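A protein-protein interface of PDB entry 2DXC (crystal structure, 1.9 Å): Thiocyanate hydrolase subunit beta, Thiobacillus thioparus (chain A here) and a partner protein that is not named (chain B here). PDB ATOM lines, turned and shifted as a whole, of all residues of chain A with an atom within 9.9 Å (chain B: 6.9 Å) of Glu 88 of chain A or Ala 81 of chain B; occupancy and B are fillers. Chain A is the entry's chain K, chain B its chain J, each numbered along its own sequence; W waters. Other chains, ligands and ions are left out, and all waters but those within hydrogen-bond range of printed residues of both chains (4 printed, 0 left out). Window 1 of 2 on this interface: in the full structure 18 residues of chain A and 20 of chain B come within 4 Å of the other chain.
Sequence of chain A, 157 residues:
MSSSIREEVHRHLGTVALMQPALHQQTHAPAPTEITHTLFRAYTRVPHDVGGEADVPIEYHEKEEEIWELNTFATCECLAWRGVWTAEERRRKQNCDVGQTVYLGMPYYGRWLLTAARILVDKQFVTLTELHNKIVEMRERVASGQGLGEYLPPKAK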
ATOM      1  N   VAL A  46       3.002   2.246  -4.086  1.00  0.00           N
ATOM      2  CA  VAL A  46       4.109   1.835  -4.937  1.00  0.00           C
ATOM      3  C   VAL A  46       4.039   2.871  -6.067  1.00  0.00           C
ATOM      4  O   VAL A  46       3.079   2.893  -6.833  1.00  0.00           O
ATOM      5  CB  VAL A  46       3.876   0.419  -5.503  1.00  0.00           C
ATOM      6  CG1 VAL A  46       5.182  -0.177  -5.935  1.00  0.00           C
ATOM      7  CG2 VAL A  46       3.218  -0.464  -4.454  1.00  0.00           C
ATOM      8  N   HIS A  48       5.037   3.284  -9.093  1.00  0.00           N
ATOM      9  CA  HIS A  48       4.745   2.923 -10.480  1.00  0.00           C
ATOM     10  C   HIS A  48       3.280   2.643 -10.810  1.00  0.00           C
ATOM     11  O   HIS A  48       2.913   2.560 -11.982  1.00  0.00           O
ATOM     12  CB  HIS A  48       5.603   1.721 -10.908  1.00  0.00           C
ATOM     13  CG  HIS A  48       5.214   0.423 -10.265  1.00  0.00           C
ATOM     14  ND1 HIS A  48       5.763  -0.785 -10.643  1.00  0.00           N
ATOM     15  CD2 HIS A  48       4.336   0.139  -9.272  1.00  0.00           C
ATOM     16  CE1 HIS A  48       5.239  -1.755  -9.914  1.00  0.00           C
ATOM     17  NE2 HIS A  48       4.371  -1.221  -9.073  1.00  0.00           N
ATOM     18  N   CYS A  76      21.718  -2.948 -18.300  1.00  0.00           N
ATOM     19  CA  CYS A  76      20.704  -3.558 -17.448  1.00  0.00           C
ATOM     20  C   CYS A  76      20.323  -4.966 -17.898  1.00  0.00           C
ATOM     21  O   CYS A  76      20.158  -5.856 -17.064  1.00  0.00           O
ATOM     22  CB  CYS A  76      19.463  -2.661 -17.374  1.00  0.00           C
ATOM     23  SG  CYS A  76      19.780  -1.091 -16.505  1.00  0.00           S
ATOM     24  N   GLU A  77      20.178  -5.179 -19.204  1.00  0.00           N
ATOM     25  CA  GLU A  77      19.837  -6.513 -19.692  1.00  0.00           C
ATOM     26  C   GLU A  77      21.030  -7.451 -19.535  1.00  0.00           C
ATOM     27  O   GLU A  77      20.858  -8.631 -19.239  1.00  0.00           O
ATOM     28  CB  GLU A  77      19.382  -6.469 -21.157  1.00  0.00           C
ATOM     29  CG  GLU A  77      17.975  -5.898 -21.349  1.00  0.00           C
ATOM     30  CD  GLU A  77      16.897  -6.750 -20.694  1.00  0.00           C
ATOM     31  OE1 GLU A  77      16.091  -7.362 -21.425  1.00  0.00           O
ATOM     32  OE2 GLU A  77      16.853  -6.807 -19.446  1.00  0.00           O
ATOM     33  N   ALA A  80      21.237  -8.688 -16.039  1.00  0.00           N
ATOM     34  CA  ALA A  80      20.209  -9.699 -15.783  1.00  0.00           C
ATOM     35  C   ALA A  80      20.603 -11.004 -16.465  1.00  0.00           C
ATOM     36  O   ALA A  80      20.500 -12.085 -15.887  1.00  0.00           O
ATOM     37  CB  ALA A  80      18.867  -9.220 -16.304  1.00  0.00           C
ATOM     38  N   VAL A  84      23.128 -11.034 -12.241  1.00  0.00           N
ATOM     39  CA  VAL A  84      23.274 -10.079 -11.147  1.00  0.00           C
ATOM     40  C   VAL A  84      21.894  -9.812 -10.538  1.00  0.00           C
ATOM     41  O   VAL A  84      21.773  -9.552  -9.341  1.00  0.00           O
ATOM     42  CB  VAL A  84      23.912  -8.766 -11.646  1.00  0.00           C
ATOM     43  CG1 VAL A  84      23.811  -7.689 -10.581  1.00  0.00           C
ATOM     44  CG2 VAL A  84      25.375  -9.012 -11.986  1.00  0.00           C
ATOM     45  N   TRP A  85      20.861  -9.889 -11.375  1.00  0.00           N
ATOM     46  CA  TRP A  85      19.475  -9.703 -10.946  1.00  0.00           C
ATOM     47  C   TRP A  85      18.509 -10.217 -12.014  1.00  0.00           C
ATOM     48  O   TRP A  85      18.914 -10.518 -13.140  1.00  0.00           O
ATOM     49  CB  TRP A  85      19.169  -8.219 -10.657  1.00  0.00           C
ATOM     50  CG  TRP A  85      19.339  -7.256 -11.830  1.00  0.00           C
ATOM     51  CD1 TRP A  85      19.682  -7.568 -13.120  1.00  0.00           C
ATOM     52  CD2 TRP A  85      19.220  -5.824 -11.787  1.00  0.00           C
ATOM     53  NE1 TRP A  85      19.790  -6.421 -13.875  1.00  0.00           N
ATOM     54  CE2 TRP A  85      19.514  -5.338 -13.082  1.00  0.00           C
ATOM     55  CE3 TRP A  85      18.895  -4.904 -10.778  1.00  0.00           C
ATOM     56  CZ2 TRP A  85      19.497  -3.970 -13.394  1.00  0.00           C
ATOM     57  CZ3 TRP A  85      18.876  -3.541 -11.090  1.00  0.00           C
ATOM     58  CH2 TRP A  85      19.176  -3.091 -12.388  1.00  0.00           C
ATOM     59  N   THR A  86      17.240 -10.349 -11.643  1.00  0.00           N
ATOM     60  CA  THR A  86      16.211 -10.750 -12.593  1.00  0.00           C
ATOM     61  C   THR A  86      15.547  -9.417 -12.938  1.00  0.00           C
ATOM     62  O   THR A  86      15.727  -8.432 -12.215  1.00  0.00           O
ATOM     63  CB  THR A  86      15.166 -11.693 -11.962  1.00  0.00           C
ATOM     64  OG1 THR A  86      14.588 -11.066 -10.812  1.00  0.00           O
ATOM     65  CG2 THR A  86      15.809 -13.017 -11.561  1.00  0.00           C
ATOM     66  N   ALA A  87      14.791  -9.374 -14.029  1.00  0.00           N
ATOM     67  CA  ALA A  87      14.133  -8.136 -14.435  1.00  0.00           C
ATOM     68  C   ALA A  87      13.165  -7.621 -13.366  1.00  0.00           C
ATOM     69  O   ALA A  87      13.028  -6.408 -13.178  1.00  0.00           O
ATOM     70  CB  ALA A  87      13.400  -8.339 -15.760  1.00  0.00           C
ATOM     71  N   GLU A  88      12.495  -8.530 -12.665  1.00  0.00           N
ATOM     72  CA  GLU A  88      11.564  -8.110 -11.626  1.00  0.00           C
ATOM     73  C   GLU A  88      12.273  -7.376 -10.487  1.00  0.00           C
ATOM     74  O   GLU A  88      11.739  -6.412  -9.941  1.00  0.00           O
ATOM     75  CB  GLU A  88      10.767  -9.305 -11.093  1.00  0.00           C
ATOM     76  CG  GLU A  88       9.424  -9.452 -11.796  1.00  0.00           C
ATOM     77  CD  GLU A  88       8.587  -8.188 -11.687  1.00  0.00           C
ATOM     78  OE1 GLU A  88       8.125  -7.673 -12.730  1.00  0.00           O
ATOM     79  OE2 GLU A  88       8.396  -7.705 -10.553  1.00  0.00           O
ATOM     80  N   GLU A  89      13.473  -7.825 -10.130  1.00  0.00           N
ATOM     81  CA  GLU A  89      14.224  -7.145  -9.082  1.00  0.00           C
ATOM     82  C   GLU A  89      14.544  -5.739  -9.583  1.00  0.00           C
ATOM     83  O   GLU A  89      14.494  -4.777  -8.817  1.00  0.00           O
ATOM     84  CB  GLU A  89      15.522  -7.898  -8.759  1.00  0.00           C
ATOM     85  CG  GLU A  89      15.312  -9.195  -7.981  1.00  0.00           C
ATOM     86  CD  GLU A  89      16.595  -9.993  -7.792  1.00  0.00           C
ATOM     87  OE1 GLU A  89      17.151 -10.484  -8.800  1.00  0.00           O
ATOM     88  OE2 GLU A  89      17.047 -10.129  -6.634  1.00  0.00           O
ATOM     89  N   ARG A  90      14.859  -5.617 -10.872  1.00  0.00           N
ATOM     90  CA  ARG A  90      15.169  -4.310 -11.450  1.00  0.00           C
ATOM     91  C   ARG A  90      13.953  -3.391 -11.380  1.00  0.00           C
ATOM     92  O   ARG A  90      14.060  -2.249 -10.940  1.00  0.00           O
ATOM     93  CB  ARG A  90      15.624  -4.438 -12.912  1.00  0.00           C
ATOM     94  CG  ARG A  90      15.851  -3.084 -13.600  1.00  0.00           C
ATOM     95  CD  ARG A  90      16.405  -3.220 -15.022  1.00  0.00           C
ATOM     96  NE  ARG A  90      15.498  -3.922 -15.932  1.00  0.00           N
ATOM     97  CZ  ARG A  90      14.289  -3.485 -16.281  1.00  0.00           C
ATOM     98  NH1 ARG A  90      13.823  -2.338 -15.798  1.00  0.00           N
ATOM     99  NH2 ARG A  90      13.543  -4.195 -17.119  1.00  0.00           N
ATOM    100  N   ARG A  91      12.799  -3.888 -11.813  1.00  0.00           N
ATOM    101  CA  ARG A  91      11.579  -3.085 -11.786  1.00  0.00           C
ATOM    102  C   ARG A  91      11.282  -2.574 -10.382  1.00  0.00           C
ATOM    103  O   ARG A  91      11.020  -1.387 -10.181  1.00  0.00           O
ATOM    104  CB  ARG A  91      10.381  -3.899 -12.298  1.00  0.00           C
ATOM    105  CG  ARG A  91      10.448  -4.217 -13.788  1.00  0.00           C
ATOM    106  CD  ARG A  91       9.106  -4.678 -14.357  1.00  0.00           C
ATOM    107  NE  ARG A  91       9.277  -5.121 -15.738  1.00  0.00           N
ATOM    108  CZ  ARG A  91       9.744  -6.318 -16.080  1.00  0.00           C
ATOM    109  NH1 ARG A  91      10.066  -7.202 -15.139  1.00  0.00           N
ATOM    110  NH2 ARG A  91       9.952  -6.615 -17.356  1.00  0.00           N
ATOM    111  N   ARG A  92      11.333  -3.474  -9.408  1.00  0.00           N
ATOM    112  CA  ARG A  92      11.062  -3.099  -8.027  1.00  0.00           C
ATOM    113  C   ARG A  92      12.013  -2.001  -7.548  1.00  0.00           C
ATOM    114  O   ARG A  92      11.583  -1.037  -6.923  1.00  0.00           O
ATOM    115  CB  ARG A  92      11.159  -4.334  -7.121  1.00  0.00           C
ATOM    116  CG  ARG A  92      10.917  -4.059  -5.637  1.00  0.00           C
ATOM    117  CD  ARG A  92      12.222  -3.797  -4.894  1.00  0.00           C
ATOM    118  NE  ARG A  92      13.093  -4.971  -4.908  1.00  0.00           N
ATOM    119  CZ  ARG A  92      14.263  -5.044  -4.280  1.00  0.00           C
ATOM    120  NH1 ARG A  92      14.710  -4.006  -3.583  1.00  0.00           N
ATOM    121  NH2 ARG A  92      14.983  -6.159  -4.340  1.00  0.00           N
ATOM    122  N   LYS A  93      13.301  -2.143  -7.846  1.00  0.00           N
ATOM    123  CA  LYS A  93      14.289  -1.149  -7.425  1.00  0.00           C
ATOM    124  C   LYS A  93      14.193   0.150  -8.226  1.00  0.00           C
ATOM    125  O   LYS A  93      14.276   1.244  -7.675  1.00  0.00           O
ATOM    126  CB  LYS A  93      15.711  -1.707  -7.575  1.00  0.00           C
ATOM    127  CG  LYS A  93      16.023  -2.920  -6.704  1.00  0.00           C
ATOM    128  CD  LYS A  93      17.442  -3.439  -6.964  1.00  0.00           C
ATOM    129  CE  LYS A  93      18.512  -2.495  -6.425  1.00  0.00           C
ATOM    130  NZ  LYS A  93      18.487  -2.412  -4.929  1.00  0.00           N
ATOM    131  N   GLN A  94      14.006   0.002  -9.533  1.00  0.00           N
ATOM    132  CA  GLN A  94      13.947   1.117 -10.473  1.00  0.00           C
ATOM    133  C   GLN A  94      12.664   1.944 -10.502  1.00  0.00           C
ATOM    134  O   GLN A  94      12.718   3.178 -10.540  1.00  0.00           O
ATOM    135  CB  GLN A  94      14.225   0.571 -11.877  1.00  0.00           C
ATOM    136  CG  GLN A  94      14.071   1.550 -13.027  1.00  0.00           C
ATOM    137  CD  GLN A  94      14.119   0.832 -14.366  1.00  0.00           C
ATOM    138  OE1 GLN A  94      15.123   0.206 -14.708  1.00  0.00           O
ATOM    139  NE2 GLN A  94      13.025   0.904 -15.124  1.00  0.00           N
ATOM    140  N   ASN A  95      11.520   1.265 -10.497  1.00  0.00           N
ATOM    141  CA  ASN A  95      10.232   1.947 -10.578  1.00  0.00           C
ATOM    142  C   ASN A  95       9.495   2.159  -9.268  1.00  0.00           C
ATOM    143  O   ASN A  95       8.455   2.819  -9.246  1.00  0.00           O
ATOM    144  CB  ASN A  95       9.316   1.196 -11.542  1.00  0.00           C
ATOM    145  CG  ASN A  95       9.993   0.886 -12.856  1.00  0.00           C
ATOM    146  OD1 ASN A  95      10.754   1.700 -13.383  1.00  0.00           O
ATOM    147  ND2 ASN A  95       9.714  -0.288 -13.400  1.00  0.00           N
ATOM    148  N   CYS A  96      10.017   1.608  -8.178  1.00  0.00           N
ATOM    149  CA  CYS A  96       9.348   1.769  -6.896  1.00  0.00           C
ATOM    150  C   CYS A  96      10.270   2.286  -5.796  1.00  0.00           C
ATOM    151  O   CYS A  96      10.001   3.331  -5.206  1.00  0.00           O
ATOM    152  CB  CYS A  96       8.716   0.440  -6.476  1.00  0.00           C
ATOM    153  SG  CYS A  96       7.602  -0.260  -7.734  1.00  0.00           S
ATOM    154  N   ASP A  97      11.362   1.569  -5.537  1.00  0.00           N
ATOM    155  CA  ASP A  97      12.300   1.961  -4.487  1.00  0.00           C
ATOM    156  C   ASP A  97      12.848   3.380  -4.618  1.00  0.00           C
ATOM    157  O   ASP A  97      13.212   3.985  -3.612  1.00  0.00           O
ATOM    158  CB  ASP A  97      13.477   0.976  -4.411  1.00  0.00           C
ATOM    159  CG  ASP A  97      13.076  -0.386  -3.855  1.00  0.00           C
ATOM    160  OD1 ASP A  97      11.895  -0.566  -3.482  1.00  0.00           O
ATOM    161  OD2 ASP A  97      13.953  -1.279  -3.790  1.00  0.00           O
ATOM    162  N   THR A 115      19.597   2.971 -11.002  1.00  0.00           N
ATOM    163  CA  THR A 115      19.311   1.665 -10.432  1.00  0.00           C
ATOM    164  C   THR A 115      20.367   0.626 -10.794  1.00  0.00           C
ATOM    165  O   THR A 115      20.663  -0.256  -9.995  1.00  0.00           O
ATOM    166  CB  THR A 115      17.905   1.202 -10.851  1.00  0.00           C
ATOM    167  OG1 THR A 115      16.955   2.213 -10.480  1.00  0.00           O
ATOM    168  CG2 THR A 115      17.531  -0.096 -10.152  1.00  0.00           C
ATOM    169  N   ILE A 119      22.254  -1.584  -7.924  1.00  0.00           N
ATOM    170  CA  ILE A 119      22.370  -3.021  -7.720  1.00  0.00           C
ATOM    171  C   ILE A 119      23.826  -3.425  -7.455  1.00  0.00           C
ATOM    172  O   ILE A 119      24.082  -4.328  -6.652  1.00  0.00           O
ATOM    173  CB  ILE A 119      21.773  -3.814  -8.928  1.00  0.00           C
ATOM    174  CG1 ILE A 119      21.502  -5.269  -8.527  1.00  0.00           C
ATOM    175  CG2 ILE A 119      22.687  -3.741 -10.124  1.00  0.00           C
ATOM    176  CD1 ILE A 119      22.733  -6.092  -8.190  1.00  0.00           C
ATOM    177  N   LYS A 123      24.259  -5.255  -3.708  1.00  0.00           N
ATOM    178  CA  LYS A 123      24.661  -6.655  -3.653  1.00  0.00           C
ATOM    179  C   LYS A 123      26.161  -6.793  -3.423  1.00  0.00           C
ATOM    180  O   LYS A 123      26.743  -7.869  -3.581  1.00  0.00           O
ATOM    181  CB  LYS A 123      24.214  -7.396  -4.919  1.00  0.00           C
ATOM    182  CG  LYS A 123      22.716  -7.696  -4.898  1.00  0.00           C
ATOM    183  CD  LYS A 123      22.268  -8.625  -6.014  1.00  0.00           C
ATOM    184  CE  LYS A 123      20.781  -8.956  -5.866  1.00  0.00           C
ATOM    185  NZ  LYS A 123      20.253  -9.829  -6.960  1.00  0.00           N
ATOM    186  N   TYR B  53       5.928  -3.431  -2.588  1.00  0.00           N
ATOM    187  CA  TYR B  53       5.796  -3.877  -3.973  1.00  0.00           C
ATOM    188  C   TYR B  53       4.544  -4.691  -4.273  1.00  0.00           C
ATOM    189  O   TYR B  53       4.040  -5.435  -3.425  1.00  0.00           O
ATOM    190  CB  TYR B  53       7.024  -4.703  -4.388  1.00  0.00           C
ATOM    191  CG  TYR B  53       7.193  -4.875  -5.892  1.00  0.00           C
ATOM    192  CD1 TYR B  53       7.372  -3.767  -6.721  1.00  0.00           C
ATOM    193  CD2 TYR B  53       7.208  -6.142  -6.477  1.00  0.00           C
ATOM    194  CE1 TYR B  53       7.566  -3.910  -8.089  1.00  0.00           C
ATOM    195  CE2 TYR B  53       7.402  -6.301  -7.854  1.00  0.00           C
ATOM    196  CZ  TYR B  53       7.582  -5.175  -8.654  1.00  0.00           C
ATOM    197  OH  TYR B  53       7.788  -5.296 -10.013  1.00  0.00           O
ATOM    198  N   ARG B  55       2.227  -5.914  -8.242  1.00  0.00           N
ATOM    199  CA  ARG B  55       2.013  -5.690  -9.663  1.00  0.00           C
ATOM    200  C   ARG B  55       0.532  -5.886  -9.982  1.00  0.00           C
ATOM    201  O   ARG B  55       0.143  -6.101 -11.130  1.00  0.00           O
ATOM    202  CB  ARG B  55       2.900  -6.606 -10.519  1.00  0.00           C
ATOM    203  CG  ARG B  55       4.396  -6.278 -10.396  1.00  0.00           C
ATOM    204  CD  ARG B  55       5.229  -6.905 -11.516  1.00  0.00           C
ATOM    205  NE  ARG B  55       5.020  -6.254 -12.809  1.00  0.00           N
ATOM    206  CZ  ARG B  55       5.550  -5.085 -13.168  1.00  0.00           C
ATOM    207  NH1 ARG B  55       6.336  -4.410 -12.333  1.00  0.00           N
ATOM    208  NH2 ARG B  55       5.296  -4.590 -14.372  1.00  0.00           N
ATOM    209  N   PRO B  75       6.583 -17.527 -10.185  1.00  0.00           N
ATOM    210  CA  PRO B  75       6.611 -17.035  -8.812  1.00  0.00           C
ATOM    211  C   PRO B  75       5.885 -15.696  -8.898  1.00  0.00           C
ATOM    212  O   PRO B  75       5.914 -15.052  -9.947  1.00  0.00           O
ATOM    213  CB  PRO B  75       8.100 -16.840  -8.548  1.00  0.00           C
ATOM    214  CG  PRO B  75       8.736 -17.901  -9.401  1.00  0.00           C
ATOM    215  CD  PRO B  75       7.945 -17.798 -10.681  1.00  0.00           C
ATOM    216  N   ALA B  76       5.215 -15.287  -7.829  1.00  0.00           N
ATOM    217  CA  ALA B  76       4.537 -13.997  -7.843  1.00  0.00           C
ATOM    218  C   ALA B  76       5.630 -12.928  -7.928  1.00  0.00           C
ATOM    219  O   ALA B  76       6.723 -13.112  -7.384  1.00  0.00           O
ATOM    220  CB  ALA B  76       3.722 -13.813  -6.571  1.00  0.00           C
ATOM    221  N   ALA B  77       5.345 -11.824  -8.610  1.00  0.00           N
ATOM    222  CA  ALA B  77       6.323 -10.746  -8.736  1.00  0.00           C
ATOM    223  C   ALA B  77       6.704 -10.250  -7.348  1.00  0.00           C
ATOM    224  O   ALA B  77       7.844  -9.850  -7.107  1.00  0.00           O
ATOM    225  CB  ALA B  77       5.745  -9.603  -9.560  1.00  0.00           C
ATOM    226  N   GLU B  78       5.740 -10.284  -6.435  1.00  0.00           N
ATOM    227  CA  GLU B  78       5.972  -9.849  -5.064  1.00  0.00           C
ATOM    228  C   GLU B  78       7.107 -10.649  -4.416  1.00  0.00           C
ATOM    229  O   GLU B  78       7.763 -10.175  -3.487  1.00  0.00           O
ATOM    230  CB  GLU B  78       4.692 -10.001  -4.231  1.00  0.00           C
ATOM    231  CG  GLU B  78       3.610  -8.960  -4.521  1.00  0.00           C
ATOM    232  CD  GLU B  78       2.832  -9.220  -5.804  1.00  0.00           C
ATOM    233  OE1 GLU B  78       3.146 -10.193  -6.523  1.00  0.00           O
ATOM    234  OE2 GLU B  78       1.893  -8.445  -6.093  1.00  0.00           O
ATOM    235  N   ASP B  79       7.335 -11.865  -4.901  1.00  0.00           N
ATOM    236  CA  ASP B  79       8.404 -12.693  -4.354  1.00  0.00           C
ATOM    237  C   ASP B  79       9.646 -12.642  -5.231  1.00  0.00           C
ATOM    238  O   ASP B  79      10.765 -12.520  -4.735  1.00  0.00           O
ATOM    239  CB  ASP B  79       7.938 -14.146  -4.196  1.00  0.00           C
ATOM    240  CG  ASP B  79       6.932 -14.312  -3.075  1.00  0.00           C
ATOM    241  OD1 ASP B  79       7.111 -13.662  -2.019  1.00  0.00           O
ATOM    242  OD2 ASP B  79       5.969 -15.092  -3.239  1.00  0.00           O
ATOM    243  N   GLU B  80       9.436 -12.723  -6.538  1.00  0.00           N
ATOM    244  CA  GLU B  80      10.530 -12.698  -7.500  1.00  0.00           C
ATOM    245  C   GLU B  80      11.357 -11.411  -7.390  1.00  0.00           C
ATOM    246  O   GLU B  80      12.585 -11.443  -7.472  1.00  0.00           O
ATOM    247  CB  GLU B  80       9.953 -12.839  -8.911  1.00  0.00           C
ATOM    248  CG  GLU B  80      10.939 -13.266  -9.979  1.00  0.00           C
ATOM    249  CD  GLU B  80      10.243 -13.633 -11.281  1.00  0.00           C
ATOM    250  OE1 GLU B  80       9.563 -12.760 -11.862  1.00  0.00           O
ATOM    251  OE2 GLU B  80      10.373 -14.798 -11.721  1.00  0.00           O
ATOM    252  N   ALA B  81      10.680 -10.285  -7.186  1.00  0.00           N
ATOM    253  CA  ALA B  81      11.349  -8.991  -7.082  1.00  0.00           C
ATOM    254  C   ALA B  81      12.267  -8.868  -5.866  1.00  0.00           C
ATOM    255  O   ALA B  81      13.035  -7.912  -5.763  1.00  0.00           O
ATOM    256  CB  ALA B  81      10.314  -7.873  -7.069  1.00  0.00           C
ATOM    257  N   PHE B  82      12.186  -9.824  -4.944  1.00  0.00           N
ATOM    258  CA  PHE B  82      13.044  -9.794  -3.766  1.00  0.00           C
ATOM    259  C   PHE B  82      13.937 -11.031  -3.678  1.00  0.00           C
ATOM    260  O   PHE B  82      14.506 -11.330  -2.627  1.00  0.00           O
ATOM    261  CB  PHE B  82      12.196  -9.617  -2.501  1.00  0.00           C
ATOM    262  CG  PHE B  82      11.670  -8.212  -2.330  1.00  0.00           C
ATOM    263  CD1 PHE B  82      12.483  -7.209  -1.806  1.00  0.00           C
ATOM    264  CD2 PHE B  82      10.387  -7.876  -2.755  1.00  0.00           C
ATOM    265  CE1 PHE B  82      12.028  -5.890  -1.712  1.00  0.00           C
ATOM    266  CE2 PHE B  82       9.922  -6.562  -2.665  1.00  0.00           C
ATOM    267  CZ  PHE B  82      10.745  -5.566  -2.142  1.00  0.00           C
ATOM    268  N   GLY B  83      14.055 -11.735  -4.802  1.00  0.00           N
ATOM    269  CA  GLY B  83      14.904 -12.912  -4.873  1.00  0.00           C
ATOM    270  C   GLY B  83      14.328 -14.193  -4.309  1.00  0.00           C
ATOM    271  O   GLY B  83      15.066 -15.139  -4.053  1.00  0.00           O
ATOM    272  N   ASN B  84      13.012 -14.234  -4.123  1.00  0.00           N
ATOM    273  CA  ASN B  84      12.349 -15.409  -3.571  1.00  0.00           C
ATOM    274  C   ASN B  84      11.527 -16.110  -4.645  1.00  0.00           C
ATOM    275  O   ASN B  84      10.423 -15.677  -4.970  1.00  0.00           O
ATOM    276  CB  ASN B  84      11.438 -14.985  -2.420  1.00  0.00           C
ATOM    277  CG  ASN B  84      12.170 -14.154  -1.375  1.00  0.00           C
ATOM    278  OD1 ASN B  84      11.697 -13.091  -0.966  1.00  0.00           O
ATOM    279  ND2 ASN B  84      13.326 -14.636  -0.937  1.00  0.00           N
ATOM    280  N   GLU B  85      12.061 -17.203  -5.183  1.00  0.00           N
ATOM    281  CA  GLU B  85      11.375 -17.939  -6.240  1.00  0.00           C
ATOM    282  C   GLU B  85      10.980 -19.357  -5.845  1.00  0.00           C
ATOM    283  O   GLU B  85      10.642 -20.168  -6.707  1.00  0.00           O
ATOM    284  CB  GLU B  85      12.268 -18.005  -7.482  1.00  0.00           C
ATOM    285  CG  GLU B  85      12.772 -16.652  -7.961  1.00  0.00           C
ATOM    286  CD  GLU B  85      13.648 -16.758  -9.200  1.00  0.00           C
ATOM    287  OE1 GLU B  85      13.941 -17.895  -9.633  1.00  0.00           O
ATOM    288  OE2 GLU B  85      14.047 -15.702  -9.738  1.00  0.00           O
HETATM  289  O   HOH W   1       7.317  -1.660 -12.776  1.00  0.00           O
HETATM  290  O   HOH W   2      11.734 -11.524 -13.501  1.00  0.00           O
HETATM  291  O   HOH W   3      14.340 -13.161  -8.670  1.00  0.00           O
HETATM  292  O   HOH W   4      16.336  -8.991  -4.373  1.00  0.00           O
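OH of Tyr 53 of chain B sits at hydrogen-bond distance from OE2 of Glu 88 of chain A, at 2.5 Å.
The guanidinium group (NE) of Arg 55 of chain B lies within salt-bridge range of the side-chain carboxylate (OE1) of Glu 88 of chain A, at 3.4 Å.
The backbone carbonyl oxygen (O) of Ala 81 of chain B lies within hydrogen-bond range of the guanidinium group (NH2) of Arg 92 of chain A.
The guanidinium group (NH1) of Arg 55 of chain B lies within hydrogen-bond range of the side-chain hydroxyl (OH) of Tyr 53 of chain B, at 2.9 Å.
The side-chain carboxylate of Glu 78 of chain B sits at hydrogen-bond distance from the backbone NH of Arg 55 of chain B, at 3.3 Å.
A ring nitrogen (ND1) of His 48 of chain A sits at hydrogen-bond distance from the side-chain sulfur (SG) of Cys 96 of chain A, at 3.5 Å.
The backbone NH (N) of Thr 86 of chain A is in hydrogen-bond range of the side-chain carboxylate (OE1) of Glu 89 of chain A.
The guanidinium group (NH1) of Arg 91 of chain A is in salt-bridge range of the side-chain carboxylate (OE1) of Glu 88 of chain A (3.1 Å).
OD2 of Asp 97 of chain A lies within salt-bridge range of NH1 of Arg 92 of chain A (2.8 Å).
Among the printed residues, merely in contact across the chains: Glu 88 of chain A with Glu 80 of chain B, Glu 88 of chain A with Ala 77 of chain B, Glu 89 of chain A with Ala 81 of chain B, Arg 91 of chain A with Arg 55 of chain B, Arg 92 of chain A with Phe 82 of chain B, Glu 88 of chain A with Ala 81 of chain B, Glu 89 of chain A with Glu 80 of chain B, Arg 92 of chain A with Tyr 53 of chain B, Cys 96 of chain A with Tyr 53 of chain B, His 48 of chain A with Tyr 53 of chain B, Thr 86 of chain A with Glu 85 of chain B, Arg 91 of chain A with Tyr 53 of chain B, His 48 of chain A with Arg 55 of chain B, Glu 89 of chain A with Gly 83 of chain B and Thr 86 of chain A with Glu 80 of chain B.
Of the printed residues of chain B, Thr 86 of chain A touches Glu 80 (3.9 Å) and Glu 85 (3.7 Å).
Of chain B, only Tyr 53, Arg 55, Ala 77, Glu 80 and Ala 81 come within 4 Å of Glu 88 of chain A.
Of the printed residues of chain B, Cys 96 of chain A touches Tyr 53.
Printed residues of chain A within 4 Å of Ala 77 of chain B: Glu 88 (3.4 Å).
Asp 79 of chain B touches none of the printed residues of chain A.
Of chain A, only Thr 86, Glu 88 and Glu 89 come within 4 Å of Glu 80 of chain B.
Of chain A, only Glu 88, Glu 89 and Arg 92 come within 4 Å of Ala 81 of chain B.
Of the printed residues of chain A, Phe 82 of chain B touches Arg 92 (3.5 Å).
Of the printed residues of chain A, Glu 85 of chain B touches Thr 86 (3.7 Å).
Printed residues of chain A that touch a printed residue of chain B: His 48, Thr 86, Glu 88, Glu 89, Arg 91, Arg 92 and Cys 96.
Hydrophobic or aromatic side chains of chain A that line the printed part of chain B: His 48.
Printed residues of chain B that touch a printed residue of chain A: Tyr 53, Arg 55, Ala 77, Glu 80, Ala 81, Phe 82, Gly 83 and Glu 85.
Hydrophobic or aromatic side chains of chain B within 4 Å of the printed part of chain A: Tyr 53, Ala 77, Ala 81 and Phe 82.
Along chain B the printed residues that touch a printed residue of chain A span positions 53 to 85.
Among the printed residues, 18 pairs touch across the chains.
Water W4 lies within hydrogen-bond range of the side-chain carboxylate (OE2) of Glu 89 of chain A (2.6 Å), the guanidinium group (NH2) of Arg 92 of chain A (3.1 Å) and the backbone carbonyl oxygen (O) of Phe 82 of chain B (3.4 Å).
Water W3 lies within hydrogen-bond range of O of Glu 80 of chain B (2.7 Å), OE2 of Glu 85 of chain B (2.8 Å) and OG1 of Thr 86 of chain A (3.0 Å).
Water W1 lies within hydrogen-bond range of ND1 of His 48 of chain A (2.8 Å), ND2 of Asn 95 of chain A (2.8 Å) and NH1 of Arg 55 of chain B (3.0 Å).
Water W2 lies within hydrogen-bond range of the side-chain carboxylate of Glu 80 of chain B (3.0 Å) and the backbone NH of Glu 88 of chain A (3.2 Å).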
